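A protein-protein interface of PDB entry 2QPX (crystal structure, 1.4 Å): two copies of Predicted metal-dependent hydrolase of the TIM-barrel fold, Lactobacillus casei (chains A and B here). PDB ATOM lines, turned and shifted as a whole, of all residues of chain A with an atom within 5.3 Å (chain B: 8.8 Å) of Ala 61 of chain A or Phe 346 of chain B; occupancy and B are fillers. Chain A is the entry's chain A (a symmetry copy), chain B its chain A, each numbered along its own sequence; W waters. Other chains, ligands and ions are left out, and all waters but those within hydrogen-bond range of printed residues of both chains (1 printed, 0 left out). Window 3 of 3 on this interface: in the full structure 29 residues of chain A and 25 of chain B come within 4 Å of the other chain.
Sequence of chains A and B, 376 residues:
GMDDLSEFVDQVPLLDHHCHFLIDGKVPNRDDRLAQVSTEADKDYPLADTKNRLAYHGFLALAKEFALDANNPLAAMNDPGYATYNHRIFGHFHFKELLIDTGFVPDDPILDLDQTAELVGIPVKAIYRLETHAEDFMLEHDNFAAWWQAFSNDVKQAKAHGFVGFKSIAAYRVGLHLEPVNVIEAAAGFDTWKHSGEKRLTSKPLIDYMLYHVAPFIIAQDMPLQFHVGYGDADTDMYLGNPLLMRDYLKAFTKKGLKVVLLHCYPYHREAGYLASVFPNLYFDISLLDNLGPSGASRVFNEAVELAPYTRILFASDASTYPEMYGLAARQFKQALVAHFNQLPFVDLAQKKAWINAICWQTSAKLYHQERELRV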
ATOM      1  N   LEU A  54       6.003 -14.432  21.119  1.00  0.00           N
ATOM      2  CA  LEU A  54       5.779 -13.321  20.222  1.00  0.00           C
ATOM      3  C   LEU A  54       6.044 -13.656  18.746  1.00  0.00           C
ATOM      4  O   LEU A  54       5.335 -13.128  17.861  1.00  0.00           O
ATOM      5  CB  LEU A  54       6.615 -12.111  20.646  1.00  0.00           C
ATOM      6  CG  LEU A  54       6.200 -10.768  20.037  1.00  0.00           C
ATOM      7  CD1 LEU A  54       4.715 -10.435  20.386  1.00  0.00           C
ATOM      8  CD2 LEU A  54       7.097  -9.619  20.526  1.00  0.00           C
ATOM      9  N   TYR A  56       5.370 -16.181  16.778  1.00  0.00           N
ATOM     10  CA  TYR A  56       4.192 -16.675  16.064  1.00  0.00           C
ATOM     11  C   TYR A  56       3.262 -15.521  15.721  1.00  0.00           C
ATOM     12  O   TYR A  56       2.725 -15.451  14.587  1.00  0.00           O
ATOM     13  CB  TYR A  56       3.480 -17.743  16.878  1.00  0.00           C
ATOM     14  CG  TYR A  56       2.111 -18.147  16.357  1.00  0.00           C
ATOM     15  CD1 TYR A  56       1.963 -18.837  15.173  1.00  0.00           C
ATOM     16  CD2 TYR A  56       0.979 -17.822  17.070  1.00  0.00           C
ATOM     17  CE1 TYR A  56       0.686 -19.206  14.725  1.00  0.00           C
ATOM     18  CE2 TYR A  56      -0.262 -18.171  16.646  1.00  0.00           C
ATOM     19  CZ  TYR A  56      -0.418 -18.886  15.487  1.00  0.00           C
ATOM     20  OH  TYR A  56      -1.711 -19.234  15.063  1.00  0.00           O
ATOM     21  N   HIS A  57       3.040 -14.649  16.689  1.00  0.00           N
ATOM     22  CA  HIS A  57       2.188 -13.481  16.420  1.00  0.00           C
ATOM     23  C   HIS A  57       2.740 -12.544  15.375  1.00  0.00           C
ATOM     24  O   HIS A  57       1.963 -11.980  14.574  1.00  0.00           O
ATOM     25  CB  HIS A  57       1.845 -12.781  17.717  1.00  0.00           C
ATOM     26  CG  HIS A  57       0.990 -13.624  18.594  1.00  0.00           C
ATOM     27  ND1 HIS A  57      -0.387 -13.577  18.571  1.00  0.00           N
ATOM     28  CD2 HIS A  57       1.314 -14.622  19.469  1.00  0.00           C
ATOM     29  CE1 HIS A  57      -0.869 -14.481  19.410  1.00  0.00           C
ATOM     30  NE2 HIS A  57       0.145 -15.129  19.970  1.00  0.00           N
ATOM     31  N   GLY A  58       4.056 -12.385  15.320  1.00  0.00           N
ATOM     32  CA  GLY A  58       4.692 -11.655  14.229  1.00  0.00           C
ATOM     33  C   GLY A  58       4.445 -12.303  12.894  1.00  0.00           C
ATOM     34  O   GLY A  58       4.167 -11.623  11.919  1.00  0.00           O
ATOM     35  N   PHE A  59       4.557 -13.621  12.847  1.00  0.00           N
ATOM     36  CA  PHE A  59       4.286 -14.331  11.591  1.00  0.00           C
ATOM     37  C   PHE A  59       2.856 -14.126  11.159  1.00  0.00           C
ATOM     38  O   PHE A  59       2.580 -13.885   9.979  1.00  0.00           O
ATOM     39  CB  PHE A  59       4.473 -15.851  11.737  1.00  0.00           C
ATOM     40  CG  PHE A  59       5.909 -16.331  11.778  1.00  0.00           C
ATOM     41  CD1 PHE A  59       6.990 -15.479  11.797  1.00  0.00           C
ATOM     42  CD2 PHE A  59       6.144 -17.680  11.798  1.00  0.00           C
ATOM     43  CE1 PHE A  59       8.286 -15.980  11.860  1.00  0.00           C
ATOM     44  CE2 PHE A  59       7.431 -18.183  11.855  1.00  0.00           C
ATOM     45  CZ  PHE A  59       8.492 -17.327  11.890  1.00  0.00           C
ATOM     46  N   LEU A  60       1.921 -14.221  12.094  1.00  0.00           N
ATOM     47  CA  LEU A  60       0.493 -13.999  11.757  1.00  0.00           C
ATOM     48  C   LEU A  60       0.241 -12.609  11.255  1.00  0.00           C
ATOM     49  O   LEU A  60      -0.575 -12.406  10.342  1.00  0.00           O
ATOM     50  CB  LEU A  60      -0.390 -14.212  12.981  1.00  0.00           C
ATOM     51  CG  LEU A  60      -0.617 -15.613  13.461  1.00  0.00           C
ATOM     52  CD1 LEU A  60      -1.680 -15.587  14.601  1.00  0.00           C
ATOM     53  CD2 LEU A  60      -1.048 -16.590  12.343  1.00  0.00           C
ATOM     54  N   ALA A  61       0.891 -11.621  11.853  1.00  0.00           N
ATOM     55  CA  ALA A  61       0.722 -10.238  11.457  1.00  0.00           C
ATOM     56  C   ALA A  61       1.160 -10.072  10.013  1.00  0.00           C
ATOM     57  O   ALA A  61       0.475  -9.412   9.220  1.00  0.00           O
ATOM     58  CB  ALA A  61       1.539  -9.285  12.397  1.00  0.00           C
ATOM     59  N   LEU A  62       2.280 -10.673   9.642  1.00  0.00           N
ATOM     60  CA  LEU A  62       2.762 -10.564   8.270  1.00  0.00           C
ATOM     61  C   LEU A  62       1.859 -11.326   7.309  1.00  0.00           C
ATOM     62  O   LEU A  62       1.577 -10.826   6.238  1.00  0.00           O
ATOM     63  CB  LEU A  62       4.227 -10.992   8.106  1.00  0.00           C
ATOM     64  CG  LEU A  62       5.292  -9.890   8.253  1.00  0.00           C
ATOM     65  CD1 LEU A  62       5.435  -9.567   9.723  1.00  0.00           C
ATOM     66  CD2 LEU A  62       6.598 -10.363   7.673  1.00  0.00           C
ATOM     67  N   ALA A  63       1.365 -12.485   7.708  1.00  0.00           N
ATOM     68  CA  ALA A  63       0.430 -13.235   6.876  1.00  0.00           C
ATOM     69  C   ALA A  63      -0.799 -12.418   6.539  1.00  0.00           C
ATOM     70  O   ALA A  63      -1.286 -12.426   5.419  1.00  0.00           O
ATOM     71  CB  ALA A  63       0.040 -14.566   7.499  1.00  0.00           C
ATOM     72  N   LYS A  64      -1.334 -11.725   7.526  1.00  0.00           N
ATOM     73  CA  LYS A  64      -2.508 -10.879   7.324  1.00  0.00           C
ATOM     74  C   LYS A  64      -2.183  -9.711   6.402  1.00  0.00           C
ATOM     75  O   LYS A  64      -2.947  -9.407   5.483  1.00  0.00           O
ATOM     76  CB  LYS A  64      -3.032 -10.376   8.678  1.00  0.00           C
ATOM     77  CG  LYS A  64      -4.142 -11.227   9.315  1.00  0.00           C
ATOM     78  CD  LYS A  64      -3.754 -12.671   9.724  1.00  0.00           C
ATOM     79  CE  LYS A  64      -4.585 -13.109  10.933  1.00  0.00           C
ATOM     80  NZ  LYS A  64      -4.428 -14.540  11.368  1.00  0.00           N
ATOM     81  N   GLU A  65      -1.061  -9.042   6.660  1.00  0.00           N
ATOM     82  CA  GLU A  65      -0.619  -7.863   5.896  1.00  0.00           C
ATOM     83  C   GLU A  65      -0.467  -8.117   4.395  1.00  0.00           C
ATOM     84  O   GLU A  65      -0.859  -7.285   3.577  1.00  0.00           O
ATOM     85  CB  GLU A  65       0.708  -7.307   6.476  1.00  0.00           C
ATOM     86  CG  GLU A  65       1.337  -6.156   5.736  1.00  0.00           C
ATOM     87  CD  GLU A  65       2.561  -5.626   6.459  1.00  0.00           C
ATOM     88  OE1 GLU A  65       2.944  -6.215   7.514  1.00  0.00           O
ATOM     89  OE2 GLU A  65       3.149  -4.626   5.996  1.00  0.00           O
ATOM     90  N   PHE A  66       0.078  -9.276   4.048  1.00  0.00           N
ATOM     91  CA  PHE A  66       0.377  -9.600   2.676  1.00  0.00           C
ATOM     92  C   PHE A  66      -0.589 -10.619   2.046  1.00  0.00           C
ATOM     93  O   PHE A  66      -0.377 -11.002   0.888  1.00  0.00           O
ATOM     94  CB  PHE A  66       1.823 -10.108   2.615  1.00  0.00           C
ATOM     95  CG  PHE A  66       2.815  -9.039   2.922  1.00  0.00           C
ATOM     96  CD1 PHE A  66       3.123  -8.055   1.980  1.00  0.00           C
ATOM     97  CD2 PHE A  66       3.458  -8.989   4.156  1.00  0.00           C
ATOM     98  CE1 PHE A  66       4.019  -7.053   2.266  1.00  0.00           C
ATOM     99  CE2 PHE A  66       4.376  -8.002   4.432  1.00  0.00           C
ATOM    100  CZ  PHE A  66       4.669  -7.042   3.500  1.00  0.00           C
ATOM    101  N   PRO A 294      11.681 -11.666  18.227  1.00  0.00           N
ATOM    102  CA  PRO A 294      11.544 -10.371  17.562  1.00  0.00           C
ATOM    103  C   PRO A 294      11.574  -9.156  18.490  1.00  0.00           C
ATOM    104  O   PRO A 294      12.088  -8.086  18.083  1.00  0.00           O
ATOM    105  CB  PRO A 294      10.207 -10.521  16.805  1.00  0.00           C
ATOM    106  CG  PRO A 294       9.458 -11.513  17.581  1.00  0.00           C
ATOM    107  CD  PRO A 294      10.474 -12.496  18.018  1.00  0.00           C
ATOM    108  N   LEU A 328       9.750 -11.373   8.573  1.00  0.00           N
ATOM    109  CA  LEU A 328       9.862 -10.901   9.965  1.00  0.00           C
ATOM    110  C   LEU A 328      11.307 -10.564  10.342  1.00  0.00           C
ATOM    111  O   LEU A 328      11.581  -9.550  10.975  1.00  0.00           O
ATOM    112  CB  LEU A 328       9.248 -11.867  10.969  1.00  0.00           C
ATOM    113  CG  LEU A 328       9.162 -11.381  12.425  1.00  0.00           C
ATOM    114  CD1 LEU A 328       8.375 -10.114  12.504  1.00  0.00           C
ATOM    115  CD2 LEU A 328       8.532 -12.471  13.313  1.00  0.00           C
ATOM    116  N   GLN A 332      12.375  -6.786  11.451  1.00  0.00           N
ATOM    117  CA  GLN A 332      12.947  -6.502  12.771  1.00  0.00           C
ATOM    118  C   GLN A 332      14.378  -5.994  12.649  1.00  0.00           C
ATOM    119  O   GLN A 332      14.813  -5.125  13.415  1.00  0.00           O
ATOM    120  CB  GLN A 332      12.902  -7.724  13.692  1.00  0.00           C
ATOM    121  CG  GLN A 332      11.490  -8.234  13.956  1.00  0.00           C
ATOM    122  CD  GLN A 332      10.517  -7.178  14.424  1.00  0.00           C
ATOM    123  OE1 GLN A 332       9.797  -6.614  13.610  1.00  0.00           O
ATOM    124  NE2 GLN A 332      10.554  -6.835  15.729  1.00  0.00           N
ATOM    125  N   GLY B   1      -1.026  -2.315  18.779  1.00  0.00           N
ATOM    126  CA  GLY B   1      -0.421  -0.955  18.748  1.00  0.00           C
ATOM    127  C   GLY B   1       0.101  -0.500  20.104  1.00  0.00           C
ATOM    128  O   GLY B   1       0.625  -1.295  20.884  1.00  0.00           O
ATOM    129  N   MET B   2      -0.031   0.797  20.363  1.00  0.00           N
ATOM    130  CA  MET B   2       0.467   1.400  21.597  1.00  0.00           C
ATOM    131  C   MET B   2      -0.684   1.524  22.568  1.00  0.00           C
ATOM    132  O   MET B   2      -1.660   2.225  22.312  1.00  0.00           O
ATOM    133  CB  MET B   2       1.062   2.776  21.333  1.00  0.00           C
ATOM    134  CG  MET B   2       1.634   3.486  22.568  1.00  0.00           C
ATOM    135  SD  MET B   2       3.155   2.657  23.525  1.00  0.00           S
ATOM    136  CE  MET B   2       4.460   2.493  21.975  1.00  0.00           C
ATOM    137  N   ASP B   3      -0.558   0.863  23.702  1.00  0.00           N
ATOM    138  CA  ASP B   3      -1.630   0.833  24.659  1.00  0.00           C
ATOM    139  C   ASP B   3      -1.184   1.549  25.908  1.00  0.00           C
ATOM    140  O   ASP B   3      -0.035   1.988  25.990  1.00  0.00           O
ATOM    141  CB  ASP B   3      -2.014  -0.605  24.915  1.00  0.00           C
ATOM    142  CG  ASP B   3      -2.698  -1.243  23.702  1.00  0.00           C
ATOM    143  OD1 ASP B   3      -3.858  -0.887  23.428  1.00  0.00           O
ATOM    144  OD2 ASP B   3      -2.104  -2.112  23.027  1.00  0.00           O
ATOM    145  N   TYR B 310       5.074 -16.253  26.967  1.00  0.00           N
ATOM    146  CA  TYR B 310       4.596 -15.411  28.044  1.00  0.00           C
ATOM    147  C   TYR B 310       3.846 -16.228  29.099  1.00  0.00           C
ATOM    148  O   TYR B 310       3.728 -15.793  30.245  1.00  0.00           O
ATOM    149  CB  TYR B 310       3.697 -14.268  27.491  1.00  0.00           C
ATOM    150  CG  TYR B 310       4.494 -13.199  26.784  1.00  0.00           C
ATOM    151  CD1 TYR B 310       5.212 -12.241  27.494  1.00  0.00           C
ATOM    152  CD2 TYR B 310       4.502 -13.099  25.388  1.00  0.00           C
ATOM    153  CE1 TYR B 310       5.970 -11.251  26.837  1.00  0.00           C
ATOM    154  CE2 TYR B 310       5.242 -12.127  24.738  1.00  0.00           C
ATOM    155  CZ  TYR B 310       5.961 -11.188  25.448  1.00  0.00           C
ATOM    156  OH  TYR B 310       6.674 -10.210  24.806  1.00  0.00           O
ATOM    157  N   PHE B 341       4.616  -4.215  27.796  1.00  0.00           N
ATOM    158  CA  PHE B 341       3.441  -4.480  26.999  1.00  0.00           C
ATOM    159  C   PHE B 341       2.840  -3.251  26.326  1.00  0.00           C
ATOM    160  O   PHE B 341       2.188  -3.409  25.276  1.00  0.00           O
ATOM    161  CB  PHE B 341       2.374  -5.202  27.798  1.00  0.00           C
ATOM    162  CG  PHE B 341       2.723  -6.637  28.082  1.00  0.00           C
ATOM    163  CD1 PHE B 341       2.720  -7.577  27.072  1.00  0.00           C
ATOM    164  CD2 PHE B 341       3.124  -7.025  29.346  1.00  0.00           C
ATOM    165  CE1 PHE B 341       3.089  -8.899  27.337  1.00  0.00           C
ATOM    166  CE2 PHE B 341       3.477  -8.323  29.617  1.00  0.00           C
ATOM    167  CZ  PHE B 341       3.461  -9.263  28.620  1.00  0.00           C
ATOM    168  N   GLN B 343       4.078  -0.985  24.403  1.00  0.00           N
ATOM    169  CA  GLN B 343       4.498  -0.778  23.011  1.00  0.00           C
ATOM    170  C   GLN B 343       4.798  -2.083  22.269  1.00  0.00           C
ATOM    171  O   GLN B 343       5.360  -2.065  21.173  1.00  0.00           O
ATOM    172  CB  GLN B 343       5.738   0.122  22.964  1.00  0.00           C
ATOM    173  N   LEU B 344       4.453  -3.206  22.864  1.00  0.00           N
ATOM    174  CA  LEU B 344       4.758  -4.499  22.248  1.00  0.00           C
ATOM    175  C   LEU B 344       3.990  -4.602  20.927  1.00  0.00           C
ATOM    176  O   LEU B 344       2.770  -4.380  20.937  1.00  0.00           O
ATOM    177  CB  LEU B 344       4.338  -5.629  23.147  1.00  0.00           C
ATOM    178  CG  LEU B 344       4.946  -6.995  22.856  1.00  0.00           C
ATOM    179  CD1 LEU B 344       6.464  -7.018  23.107  1.00  0.00           C
ATOM    180  CD2 LEU B 344       4.189  -8.002  23.670  1.00  0.00           C
ATOM    181  N   PRO B 345       4.684  -4.964  19.814  1.00  0.00           N
ATOM    182  CA  PRO B 345       4.041  -5.094  18.483  1.00  0.00           C
ATOM    183  C   PRO B 345       3.187  -6.354  18.319  1.00  0.00           C
ATOM    184  O   PRO B 345       3.225  -7.265  19.133  1.00  0.00           O
ATOM    185  CB  PRO B 345       5.226  -5.162  17.534  1.00  0.00           C
ATOM    186  CG  PRO B 345       6.325  -5.784  18.341  1.00  0.00           C
ATOM    187  CD  PRO B 345       6.126  -5.247  19.742  1.00  0.00           C
ATOM    188  N   PHE B 346       2.413  -6.372  17.234  1.00  0.00           N
ATOM    189  CA  PHE B 346       1.764  -7.565  16.667  1.00  0.00           C
ATOM    190  C   PHE B 346       0.472  -7.973  17.358  1.00  0.00           C
ATOM    191  O   PHE B 346      -0.420  -8.519  16.724  1.00  0.00           O
ATOM    192  CB  PHE B 346       2.695  -8.799  16.553  1.00  0.00           C
ATOM    193  CG  PHE B 346       4.024  -8.513  15.938  1.00  0.00           C
ATOM    194  CD1 PHE B 346       4.129  -7.792  14.776  1.00  0.00           C
ATOM    195  CD2 PHE B 346       5.199  -8.973  16.550  1.00  0.00           C
ATOM    196  CE1 PHE B 346       5.360  -7.521  14.231  1.00  0.00           C
ATOM    197  CE2 PHE B 346       6.411  -8.705  15.980  1.00  0.00           C
ATOM    198  CZ  PHE B 346       6.497  -7.987  14.841  1.00  0.00           C
ATOM    199  N   VAL B 347       0.342  -7.741  18.653  1.00  0.00           N
ATOM    200  CA  VAL B 347      -0.743  -8.334  19.411  1.00  0.00           C
ATOM    201  C   VAL B 347      -1.708  -7.228  19.843  1.00  0.00           C
ATOM    202  O   VAL B 347      -1.321  -6.055  20.032  1.00  0.00           O
ATOM    203  CB  VAL B 347      -0.217  -9.122  20.665  1.00  0.00           C
ATOM    204  CG1 VAL B 347       0.582 -10.341  20.206  1.00  0.00           C
ATOM    205  CG2 VAL B 347       0.562  -8.211  21.595  1.00  0.00           C
ATOM    206  N   ASP B 348      -2.946  -7.632  20.052  1.00  0.00           N
ATOM    207  CA  ASP B 348      -3.978  -6.685  20.423  1.00  0.00           C
ATOM    208  C   ASP B 348      -4.013  -6.492  21.929  1.00  0.00           C
ATOM    209  O   ASP B 348      -3.315  -7.184  22.705  1.00  0.00           O
ATOM    210  CB  ASP B 348      -5.374  -7.013  19.807  1.00  0.00           C
ATOM    211  CG  ASP B 348      -5.937  -8.349  20.225  1.00  0.00           C
ATOM    212  OD1 ASP B 348      -5.497  -8.962  21.235  1.00  0.00           O
ATOM    213  OD2 ASP B 348      -6.853  -8.829  19.503  1.00  0.00           O
ATOM    214  N   LEU B 349      -4.778  -5.500  22.357  1.00  0.00           N
ATOM    215  CA  LEU B 349      -4.906  -5.221  23.765  1.00  0.00           C
ATOM    216  C   LEU B 349      -5.375  -6.428  24.578  1.00  0.00           C
ATOM    217  O   LEU B 349      -4.844  -6.696  25.668  1.00  0.00           O
ATOM    218  CB  LEU B 349      -5.862  -4.023  23.965  1.00  0.00           C
ATOM    219  CG  LEU B 349      -6.022  -3.583  25.428  1.00  0.00           C
ATOM    220  CD1 LEU B 349      -4.669  -3.199  26.100  1.00  0.00           C
ATOM    221  CD2 LEU B 349      -7.073  -2.421  25.529  1.00  0.00           C
ATOM    222  N   GLN B 351      -4.905  -9.566  24.044  1.00  0.00           N
ATOM    223  CA  GLN B 351      -3.791 -10.537  24.189  1.00  0.00           C
ATOM    224  C   GLN B 351      -2.788 -10.057  25.225  1.00  0.00           C
ATOM    225  O   GLN B 351      -2.264 -10.864  26.032  1.00  0.00           O
ATOM    226  CB  GLN B 351      -3.130 -10.774  22.834  1.00  0.00           C
ATOM    227  CG  GLN B 351      -1.996 -11.805  22.870  1.00  0.00           C
ATOM    228  CD  GLN B 351      -2.454 -13.145  23.273  1.00  0.00           C
ATOM    229  OE1 GLN B 351      -2.939 -13.945  22.430  1.00  0.00           O
ATOM    230  NE2 GLN B 351      -2.285 -13.464  24.568  1.00  0.00           N
ATOM    231  N   LYS B 352      -2.503  -8.757  25.206  1.00  0.00           N
ATOM    232  CA  LYS B 352      -1.645  -8.171  26.239  1.00  0.00           C
ATOM    233  C   LYS B 352      -2.198  -8.443  27.653  1.00  0.00           C
ATOM    234  O   LYS B 352      -1.470  -8.868  28.567  1.00  0.00           O
ATOM    235  CB  LYS B 352      -1.408  -6.685  25.969  1.00  0.00           C
ATOM    236  CG  LYS B 352      -0.691  -6.375  24.645  1.00  0.00           C
ATOM    237  CD  LYS B 352      -0.550  -4.863  24.368  1.00  0.00           C
ATOM    238  CE  LYS B 352       0.163  -4.562  23.095  1.00  0.00           C
ATOM    239  NZ  LYS B 352       0.471  -3.084  22.938  1.00  0.00           N
ATOM    240  N   TRP B 355      -1.884 -12.154  28.651  1.00  0.00           N
ATOM    241  CA  TRP B 355      -0.519 -12.490  29.048  1.00  0.00           C
ATOM    242  C   TRP B 355      -0.159 -11.923  30.417  1.00  0.00           C
ATOM    243  O   TRP B 355       0.455 -12.623  31.264  1.00  0.00           O
ATOM    244  CB  TRP B 355       0.445 -12.046  27.965  1.00  0.00           C
ATOM    245  CG  TRP B 355       0.477 -12.956  26.750  1.00  0.00           C
ATOM    246  CD1 TRP B 355       0.130 -14.268  26.704  1.00  0.00           C
ATOM    247  CD2 TRP B 355       0.984 -12.625  25.467  1.00  0.00           C
ATOM    248  NE1 TRP B 355       0.392 -14.785  25.450  1.00  0.00           N
ATOM    249  CE2 TRP B 355       0.940 -13.806  24.679  1.00  0.00           C
ATOM    250  CE3 TRP B 355       1.511 -11.461  24.908  1.00  0.00           C
ATOM    251  CZ2 TRP B 355       1.340 -13.832  23.356  1.00  0.00           C
ATOM    252  CZ3 TRP B 355       1.915 -11.498  23.565  1.00  0.00           C
ATOM    253  CH2 TRP B 355       1.853 -12.683  22.833  1.00  0.00           C
HETATM  254  O   HOH W   1      -0.628 -10.932  15.155  1.00  0.00           O
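O of Leu 344 of chain B sits at hydrogen-bond distance from NZ of Lys 352 of chain B, at 3.3 Å. The side-chain carboxylate of Asp 348 of chain B lies within hydrogen-bond range of the backbone NH of Gln 351 of chain B. The indole nitrogen (NE1) of Trp 355 of chain B lies close to the side-chain amide nitrogen (NE2) of Gln 351 of chain B (3.1 Å). The backbone carbonyl oxygen (O) of Pro 294 of chain A sits at hydrogen-bond distance from the side-chain amide nitrogen (NE2) of Gln 332 of chain A.
CD1 of Leu 344 of chain B touches CD2 of Leu 54 of chain A, at 3.7 Å. O of Pro 345 of chain B touches CD1 of Leu 54 of chain A, at 3.7 Å. His 57 of chain A touches Phe 346 of chain B. CG of His 57 of chain A touches CG1 of Val 347 of chain B, 3.7 Å away. His 57 of chain A touches Gln 351 of chain B. NE2 of His 57 of chain A touches CZ2 of Trp 355 of chain B (3.8 Å). CD2 of Phe 346 of chain B touches CA of Gly 58 of chain A, 3.6 Å away. Ala 61 of chain A touches Phe 346 of chain B. Leu 328 of chain A touches Phe 346 of chain B (CD1 to CZ, 3.7 Å). Phe 346 of chain B touches Gln 332 of chain A (CZ to OE1, 3.8 Å).
Printed residues of chain B within 4 Å of Ala 61 of chain A: Phe 346. Printed residues of chain A within 4 Å of Phe 346 of chain B: His 57, Gly 58, Ala 61, Leu 328 and Gln 332. Of the printed residues of chain B, Gly 58 of chain A touches Phe 346 (3.6 Å). Printed residues of chain B within 4 Å of His 57 of chain A: Phe 346 (3.8 Å), Val 347 (3.7 Å), Gln 351 (3.7 Å) and Trp 355 (3.8 Å). Of the printed residues of chain A, Leu 344 of chain B touches Leu 54. The nearest printed residue of chain A that does not touch Phe 346 of chain B is Leu 54 of chain A (4.05 Å).
Printed residues of chain B that touch a printed residue of chain A: Leu 344, Pro 345, Phe 346, Val 347, Gln 351 and Trp 355. Hydrophobic or aromatic side chains of chain B that line the printed part of chain A: Leu 344, Phe 346, Val 347 and Trp 355. Along chain B the printed residues that touch a printed residue of chain A span positions 344 to 355. Of the 15 printed residues of chain A, 6 touch a printed residue of chain B. Among the printed residues, no Asp or Glu carboxylate lies within 4 Å of a Lys or Arg side-chain nitrogen of the other chain.
No position is printed for both chains. Of the 10 pairs that touch across the chains among the printed residues, none has its exchanged pair printed and touching as well.
Water W1 bridges the backbone carbonyl oxygen of His 57 of chain A (2.9 Å) and the backbone carbonyl oxygen of Phe 346 of chain B (2.9 Å).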
